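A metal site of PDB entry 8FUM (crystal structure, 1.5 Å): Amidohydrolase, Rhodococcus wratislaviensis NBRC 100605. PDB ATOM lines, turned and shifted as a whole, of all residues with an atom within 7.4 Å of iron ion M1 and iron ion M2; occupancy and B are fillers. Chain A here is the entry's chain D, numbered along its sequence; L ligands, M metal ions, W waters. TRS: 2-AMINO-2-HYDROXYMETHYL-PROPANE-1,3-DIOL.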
ATOM      1  N   ASP A  25     -16.648   8.928  10.730  1.00  0.00           N
ATOM      2  CA  ASP A  25     -16.561   7.580  11.313  1.00  0.00           C
ATOM      3  C   ASP A  25     -17.842   7.269  12.077  1.00  0.00           C
ATOM      4  O   ASP A  25     -18.014   7.705  13.225  1.00  0.00           O
ATOM      5  CB  ASP A  25     -15.330   7.478  12.210  1.00  0.00           C
ATOM      6  CG  ASP A  25     -15.012   6.053  12.609  1.00  0.00           C
ATOM      7  OD1 ASP A  25     -15.377   5.161  11.824  1.00  0.00           O
ATOM      8  OD2 ASP A  25     -14.427   5.833  13.687  1.00  0.00           O
ATOM      9  N   ILE A  26     -18.686   6.462  11.447  1.00  0.00           N
ATOM     10  CA  ILE A  26     -19.934   5.950  12.008  1.00  0.00           C
ATOM     11  C   ILE A  26     -19.893   4.438  11.892  1.00  0.00           C
ATOM     12  O   ILE A  26     -19.463   3.913  10.862  1.00  0.00           O
ATOM     13  CB  ILE A  26     -21.130   6.492  11.199  1.00  0.00           C
ATOM     14  CG1 ILE A  26     -21.134   8.014  11.232  1.00  0.00           C
ATOM     15  CG2 ILE A  26     -22.422   5.926  11.733  1.00  0.00           C
ATOM     16  CD1 ILE A  26     -22.122   8.619  10.263  1.00  0.00           C
ATOM     17  N   HIS A  27     -20.335   3.735  12.937  1.00  0.00           N
ATOM     18  CA  HIS A  27     -20.217   2.272  12.962  1.00  0.00           C
ATOM     19  C   HIS A  27     -21.559   1.549  12.943  1.00  0.00           C
ATOM     20  O   HIS A  27     -22.092   1.181  13.998  1.00  0.00           O
ATOM     21  CB  HIS A  27     -19.362   1.826  14.154  1.00  0.00           C
ATOM     22  CG  HIS A  27     -17.958   2.340  14.066  1.00  0.00           C
ATOM     23  ND1 HIS A  27     -17.161   2.096  12.973  1.00  0.00           N
ATOM     24  CD2 HIS A  27     -17.219   3.106  14.901  1.00  0.00           C
ATOM     25  CE1 HIS A  27     -15.998   2.698  13.129  1.00  0.00           C
ATOM     26  NE2 HIS A  27     -15.998   3.302  14.301  1.00  0.00           N
ATOM     27  N   ALA A  71     -18.000  -1.422  25.146  1.00  0.00           N
ATOM     28  CA  ALA A  71     -17.473  -0.123  24.741  1.00  0.00           C
ATOM     29  C   ALA A  71     -18.480   0.681  23.925  1.00  0.00           C
ATOM     30  O   ALA A  71     -18.102   1.548  23.132  1.00  0.00           O
ATOM     31  CB  ALA A  71     -16.140  -0.254  23.986  1.00  0.00           C
ATOM     32  N   GLN A 106     -18.269   2.956   8.482  1.00  0.00           N
ATOM     33  CA  GLN A 106     -17.090   2.098   8.568  1.00  0.00           C
ATOM     34  C   GLN A 106     -17.566   0.847   9.313  1.00  0.00           C
ATOM     35  O   GLN A 106     -17.625   0.819  10.545  1.00  0.00           O
ATOM     36  CB  GLN A 106     -15.950   2.819   9.286  1.00  0.00           C
ATOM     37  CG  GLN A 106     -15.572   4.140   8.616  1.00  0.00           C
ATOM     38  CD  GLN A 106     -14.203   4.661   9.010  1.00  0.00           C
ATOM     39  OE1 GLN A 106     -13.329   3.900   9.432  1.00  0.00           O
ATOM     40  NE2 GLN A 106     -13.999   5.976   8.864  1.00  0.00           N
ATOM     41  N   LEU A 108     -17.175  -2.354  11.037  1.00  0.00           N
ATOM     42  CA  LEU A 108     -16.057  -3.009  11.724  1.00  0.00           C
ATOM     43  C   LEU A 108     -16.322  -4.461  12.083  1.00  0.00           C
ATOM     44  O   LEU A 108     -15.453  -5.102  12.687  1.00  0.00           O
ATOM     45  CB  LEU A 108     -15.766  -2.271  13.038  1.00  0.00           C
ATOM     46  CG  LEU A 108     -15.375  -0.788  12.960  1.00  0.00           C
ATOM     47  CD1 LEU A 108     -15.145  -0.238  14.370  1.00  0.00           C
ATOM     48  CD2 LEU A 108     -14.122  -0.622  12.082  1.00  0.00           C
ATOM     49  N   THR A 114     -18.362  -5.274  18.382  1.00  0.00           N
ATOM     50  CA  THR A 114     -17.810  -3.932  18.327  1.00  0.00           C
ATOM     51  C   THR A 114     -16.674  -3.788  17.312  1.00  0.00           C
ATOM     52  O   THR A 114     -16.658  -2.819  16.546  1.00  0.00           O
ATOM     53  CB  THR A 114     -17.340  -3.498  19.720  1.00  0.00           C
ATOM     54  OG1 THR A 114     -18.459  -3.540  20.622  1.00  0.00           O
ATOM     55  CG2 THR A 114     -16.795  -2.055  19.674  1.00  0.00           C
ATOM     56  N   LEU A 115     -15.724  -4.733  17.305  1.00  0.00           N
ATOM     57  CA  LEU A 115     -14.543  -4.610  16.443  1.00  0.00           C
ATOM     58  C   LEU A 115     -14.032  -6.008  16.081  1.00  0.00           C
ATOM     59  O   LEU A 115     -13.318  -6.628  16.874  1.00  0.00           O
ATOM     60  CB  LEU A 115     -13.461  -3.807  17.168  1.00  0.00           C
ATOM     61  CG  LEU A 115     -12.111  -3.642  16.491  1.00  0.00           C
ATOM     62  CD1 LEU A 115     -12.228  -2.912  15.179  1.00  0.00           C
ATOM     63  CD2 LEU A 115     -11.170  -2.922  17.485  1.00  0.00           C
ATOM     64  N   HIS A 211      -8.916   2.634   9.659  1.00  0.00           N
ATOM     65  CA  HIS A 211      -9.521   2.719  10.977  1.00  0.00           C
ATOM     66  C   HIS A 211      -8.760   1.857  11.977  1.00  0.00           C
ATOM     67  O   HIS A 211      -8.287   0.757  11.655  1.00  0.00           O
ATOM     68  CB  HIS A 211     -10.999   2.284  10.934  1.00  0.00           C
ATOM     69  CG  HIS A 211     -11.760   2.526  12.203  1.00  0.00           C
ATOM     70  ND1 HIS A 211     -11.616   1.725  13.313  1.00  0.00           N
ATOM     71  CD2 HIS A 211     -12.662   3.486  12.542  1.00  0.00           C
ATOM     72  CE1 HIS A 211     -12.405   2.169  14.283  1.00  0.00           C
ATOM     73  NE2 HIS A 211     -13.047   3.237  13.842  1.00  0.00           N
ATOM     74  N   LEU A 212      -8.615   2.383  13.185  1.00  0.00           N
ATOM     75  CA  LEU A 212      -8.118   1.636  14.323  1.00  0.00           C
ATOM     76  C   LEU A 212      -8.552   0.176  14.265  1.00  0.00           C
ATOM     77  O   LEU A 212      -9.722  -0.138  13.997  1.00  0.00           O
ATOM     78  CB  LEU A 212      -8.667   2.311  15.581  1.00  0.00           C
ATOM     79  CG  LEU A 212      -8.649   1.745  16.969  1.00  0.00           C
ATOM     80  CD1 LEU A 212      -8.991   2.893  17.941  1.00  0.00           C
ATOM     81  CD2 LEU A 212      -9.635   0.613  17.134  1.00  0.00           C
ATOM     82  N   HIS A 233      -5.748   0.818  24.819  1.00  0.00           N
ATOM     83  CA  HIS A 233      -6.475   1.863  24.131  1.00  0.00           C
ATOM     84  C   HIS A 233      -5.546   3.034  23.771  1.00  0.00           C
ATOM     85  O   HIS A 233      -5.560   3.503  22.622  1.00  0.00           O
ATOM     86  CB  HIS A 233      -7.691   2.254  24.973  1.00  0.00           C
ATOM     87  CG  HIS A 233      -8.721   3.031  24.205  1.00  0.00           C
ATOM     88  ND1 HIS A 233      -9.977   3.292  24.720  1.00  0.00           N
ATOM     89  CD2 HIS A 233      -8.686   3.635  22.992  1.00  0.00           C
ATOM     90  CE1 HIS A 233     -10.665   4.019  23.865  1.00  0.00           C
ATOM     91  NE2 HIS A 233      -9.911   4.246  22.811  1.00  0.00           N
ATOM     92  N   VAL A 264      -7.936   7.211  10.863  1.00  0.00           N
ATOM     93  CA  VAL A 264      -9.208   7.333  11.556  1.00  0.00           C
ATOM     94  C   VAL A 264      -9.066   6.703  12.936  1.00  0.00           C
ATOM     95  O   VAL A 264      -8.872   5.495  13.061  1.00  0.00           O
ATOM     96  CB  VAL A 264     -10.369   6.710  10.754  1.00  0.00           C
ATOM     97  CG1 VAL A 264     -11.680   6.813  11.566  1.00  0.00           C
ATOM     98  CG2 VAL A 264     -10.539   7.389   9.403  1.00  0.00           C
ATOM     99  N   GLU A 265      -9.225   7.540  13.963  1.00  0.00           N
ATOM    100  CA  GLU A 265      -9.255   7.109  15.356  1.00  0.00           C
ATOM    101  C   GLU A 265      -7.865   6.739  15.843  1.00  0.00           C
ATOM    102  O   GLU A 265      -7.710   5.892  16.731  1.00  0.00           O
ATOM    103  CB  GLU A 265     -10.302   6.026  15.615  1.00  0.00           C
ATOM    104  CG  GLU A 265     -10.869   6.052  17.016  1.00  0.00           C
ATOM    105  CD  GLU A 265     -12.161   5.318  17.131  1.00  0.00           C
ATOM    106  OE1 GLU A 265     -12.892   5.315  16.131  1.00  0.00           O
ATOM    107  OE2 GLU A 265     -12.416   4.743  18.214  1.00  0.00           O
ATOM    108  N   GLN A 309     -11.879  12.160  16.423  1.00  0.00           N
ATOM    109  CA  GLN A 309     -12.317  11.421  17.595  1.00  0.00           C
ATOM    110  C   GLN A 309     -11.308  10.339  17.957  1.00  0.00           C
ATOM    111  O   GLN A 309     -10.732   9.701  17.073  1.00  0.00           O
ATOM    112  CB  GLN A 309     -13.693  10.795  17.325  1.00  0.00           C
ATOM    113  CG  GLN A 309     -14.345  10.091  18.494  1.00  0.00           C
ATOM    114  CD  GLN A 309     -13.815   8.700  18.729  1.00  0.00           C
ATOM    115  OE1 GLN A 309     -13.184   8.121  17.848  1.00  0.00           O
ATOM    116  NE2 GLN A 309     -14.076   8.146  19.899  1.00  0.00           N
ATOM    117  N   PRO A 310     -11.041  10.104  19.244  1.00  0.00           N
ATOM    118  CA  PRO A 310     -11.506  10.844  20.416  1.00  0.00           C
ATOM    119  C   PRO A 310     -10.679  12.101  20.588  1.00  0.00           C
ATOM    120  O   PRO A 310      -9.451  12.036  20.616  1.00  0.00           O
ATOM    121  CB  PRO A 310     -11.282   9.855  21.561  1.00  0.00           C
ATOM    122  CG  PRO A 310     -10.068   9.067  21.133  1.00  0.00           C
ATOM    123  CD  PRO A 310     -10.192   8.957  19.623  1.00  0.00           C
ATOM    124  N   ALA A 335     -15.219  13.540  13.315  1.00  0.00           N
ATOM    125  CA  ALA A 335     -15.939  12.279  13.402  1.00  0.00           C
ATOM    126  C   ALA A 335     -16.577  12.157  14.778  1.00  0.00           C
ATOM    127  O   ALA A 335     -16.038  12.657  15.769  1.00  0.00           O
ATOM    128  CB  ALA A 335     -15.000  11.085  13.158  1.00  0.00           C
ATOM    129  N   THR A 336     -17.707  11.457  14.857  1.00  0.00           N
ATOM    130  CA  THR A 336     -18.323  11.202  16.155  1.00  0.00           C
ATOM    131  C   THR A 336     -17.922   9.863  16.765  1.00  0.00           C
ATOM    132  O   THR A 336     -17.865   9.759  17.992  1.00  0.00           O
ATOM    133  CB  THR A 336     -19.867  11.170  16.120  1.00  0.00           C
ATOM    134  OG1 THR A 336     -20.328  10.086  15.307  1.00  0.00           O
ATOM    135  CG2 THR A 336     -20.490  12.486  15.655  1.00  0.00           C
ATOM    136  N   ASP A 337     -17.692   8.837  15.941  1.00  0.00           N
ATOM    137  CA  ASP A 337     -17.518   7.443  16.372  1.00  0.00           C
ATOM    138  C   ASP A 337     -18.803   6.824  16.922  1.00  0.00           C
ATOM    139  O   ASP A 337     -18.746   5.870  17.698  1.00  0.00           O
ATOM    140  CB  ASP A 337     -16.368   7.286  17.366  1.00  0.00           C
ATOM    141  CG  ASP A 337     -15.772   5.891  17.348  1.00  0.00           C
ATOM    142  OD1 ASP A 337     -15.765   5.324  16.248  1.00  0.00           O
ATOM    143  OD2 ASP A 337     -15.323   5.387  18.404  1.00  0.00           O
ATOM    144  N   TYR A 338     -19.966   7.336  16.547  1.00  0.00           N
ATOM    145  CA  TYR A 338     -21.206   6.722  16.977  1.00  0.00           C
ATOM    146  C   TYR A 338     -21.229   5.250  16.578  1.00  0.00           C
ATOM    147  O   TYR A 338     -20.922   4.915  15.426  1.00  0.00           O
ATOM    148  CB  TYR A 338     -22.383   7.435  16.300  1.00  0.00           C
ATOM    149  CG  TYR A 338     -23.731   6.885  16.705  1.00  0.00           C
ATOM    150  CD1 TYR A 338     -24.385   7.337  17.840  1.00  0.00           C
ATOM    151  CD2 TYR A 338     -24.350   5.896  15.939  1.00  0.00           C
ATOM    152  CE1 TYR A 338     -25.604   6.813  18.233  1.00  0.00           C
ATOM    153  CE2 TYR A 338     -25.594   5.359  16.320  1.00  0.00           C
ATOM    154  CZ  TYR A 338     -26.210   5.823  17.464  1.00  0.00           C
ATOM    155  OH  TYR A 338     -27.433   5.328  17.861  1.00  0.00           O
ATOM    156  N   PRO A 339     -21.631   4.334  17.469  1.00  0.00           N
ATOM    157  CA  PRO A 339     -22.150   4.543  18.830  1.00  0.00           C
ATOM    158  C   PRO A 339     -21.200   4.161  19.964  1.00  0.00           C
ATOM    159  O   PRO A 339     -21.656   3.760  21.021  1.00  0.00           O
ATOM    160  CB  PRO A 339     -23.377   3.618  18.844  1.00  0.00           C
ATOM    161  CG  PRO A 339     -22.988   2.471  17.899  1.00  0.00           C
ATOM    162  CD  PRO A 339     -21.873   2.949  17.022  1.00  0.00           C
ATOM    163  N   HIS A 340     -19.899   4.334  19.771  1.00  0.00           N
ATOM    164  CA  HIS A 340     -18.942   3.905  20.791  1.00  0.00           C
ATOM    165  C   HIS A 340     -18.971   4.828  22.011  1.00  0.00           C
ATOM    166  O   HIS A 340     -19.409   5.969  21.951  1.00  0.00           O
ATOM    167  CB  HIS A 340     -17.545   3.802  20.199  1.00  0.00           C
ATOM    168  CG  HIS A 340     -17.416   2.720  19.169  1.00  0.00           C
ATOM    169  ND1 HIS A 340     -16.222   2.410  18.557  1.00  0.00           N
ATOM    170  CD2 HIS A 340     -18.340   1.851  18.688  1.00  0.00           C
ATOM    171  CE1 HIS A 340     -16.425   1.401  17.716  1.00  0.00           C
ATOM    172  NE2 HIS A 340     -17.701   1.047  17.776  1.00  0.00           N
ATOM    173  N   PHE A 341     -18.462   4.316  23.127  1.00  0.00           N
ATOM    174  CA  PHE A 341     -18.657   5.020  24.386  1.00  0.00           C
ATOM    175  C   PHE A 341     -17.962   6.366  24.413  1.00  0.00           C
ATOM    176  O   PHE A 341     -18.443   7.286  25.109  1.00  0.00           O
ATOM    177  CB  PHE A 341     -18.183   4.166  25.557  1.00  0.00           C
ATOM    178  CG  PHE A 341     -16.703   4.234  25.805  1.00  0.00           C
ATOM    179  CD1 PHE A 341     -15.846   3.457  25.071  1.00  0.00           C
ATOM    180  CD2 PHE A 341     -16.200   5.058  26.803  1.00  0.00           C
ATOM    181  CE1 PHE A 341     -14.472   3.525  25.283  1.00  0.00           C
ATOM    182  CE2 PHE A 341     -14.843   5.142  27.034  1.00  0.00           C
ATOM    183  CZ  PHE A 341     -13.975   4.361  26.281  1.00  0.00           C
ATOM    184  N   ASP A 342     -16.833   6.505  23.711  1.00  0.00           N
ATOM    185  CA  ASP A 342     -16.086   7.749  23.663  1.00  0.00           C
ATOM    186  C   ASP A 342     -16.487   8.639  22.482  1.00  0.00           C
ATOM    187  O   ASP A 342     -15.684   9.466  22.016  1.00  0.00           O
ATOM    188  CB  ASP A 342     -14.566   7.492  23.750  1.00  0.00           C
ATOM    189  CG  ASP A 342     -14.047   6.583  22.670  1.00  0.00           C
ATOM    190  OD1 ASP A 342     -14.833   5.955  21.934  1.00  0.00           O
ATOM    191  OD2 ASP A 342     -12.799   6.478  22.575  1.00  0.00           O
ATOM    192  N   PHE A 343     -17.707   8.453  21.985  1.00  0.00           N
ATOM    193  CA  PHE A 343     -18.362   9.362  21.045  1.00  0.00           C
ATOM    194  C   PHE A 343     -18.052  10.812  21.362  1.00  0.00           C
ATOM    195  O   PHE A 343     -18.094  11.227  22.520  1.00  0.00           O
ATOM    196  CB  PHE A 343     -19.868   9.108  21.240  1.00  0.00           C
ATOM    197  CG  PHE A 343     -20.776  10.125  20.597  1.00  0.00           C
ATOM    198  CD1 PHE A 343     -21.212  11.242  21.270  1.00  0.00           C
ATOM    199  CD2 PHE A 343     -21.252   9.905  19.312  1.00  0.00           C
ATOM    200  CE1 PHE A 343     -22.063  12.162  20.663  1.00  0.00           C
ATOM    201  CE2 PHE A 343     -22.104  10.800  18.707  1.00  0.00           C
ATOM    202  CZ  PHE A 343     -22.507  11.934  19.396  1.00  0.00           C
HETATM  203  C   TRS L   1     -13.002   1.724  20.568  1.00  0.00           C
HETATM  204  C1  TRS L   1     -13.363   2.985  21.337  1.00  0.00           C
HETATM  205  C2  TRS L   1     -14.097   0.662  20.703  1.00  0.00           C
HETATM  206  C3  TRS L   1     -11.664   1.185  21.063  1.00  0.00           C
HETATM  207  N   TRS L   1     -12.880   2.050  19.122  1.00  0.00           N
HETATM  208  O1  TRS L   1     -14.199   3.813  20.548  1.00  0.00           O
HETATM  209  O2  TRS L   1     -13.875  -0.355  19.737  1.00  0.00           O
HETATM  210  O3  TRS L   1     -11.744   0.911  22.443  1.00  0.00           O
HETATM  211 FE    FE M   1     -14.371   4.296  15.120  1.00  0.00          FE
HETATM  212 FE    FE M   2     -14.302   3.597  18.416  1.00  0.00          FE
HETATM  213  O   HOH W   1     -14.137   2.883  16.632  1.00  0.00           O
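The side-chain amide nitrogen of Gln 309 lies close to the side-chain carboxylate of Asp 337.
The side-chain carboxylate (OE1) of Glu 265 lies close to the side-chain amide oxygen (OE1) of Gln 309, 3.3 Å away.
A ring nitrogen (ND1) of His 27 is in hydrogen-bond range of the backbone carbonyl oxygen (O) of Gln 106 (2.8 Å).
The backbone NH (N) of His 27 is in hydrogen-bond range of the backbone carbonyl oxygen (O) of Tyr 338.
The side-chain carboxylate (OD1) of Asp 25 sits close to the side-chain amide nitrogen (NE2) of Gln 106, 3.4 Å away.
Of the 24 residues printed, 5 come within 4 Å of iron ion M1.
Iron ion M1 is bound by the side-chain carboxylate of Glu 265, the side-chain carboxylate of Asp 337, a ring nitrogen (NE2) of His 27, water W1, the side-chain carboxylate of Asp 25 and a ring nitrogen (NE2) of His 211.
Iron ion M2 is bound by water W1 (1.9 Å), the side-chain carboxylate (OD2) of Asp 337 (2.1 Å), an oxygen (O1) of the ligand (2.1 Å), the side-chain carboxylate (OE2) of Glu 265 (2.2 Å), a nitrogen (N) of the ligand (2.2 Å) and a ring nitrogen (ND1) of His 340 (2.3 Å).
Iron ion M2 has six donor atoms within binding distance.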
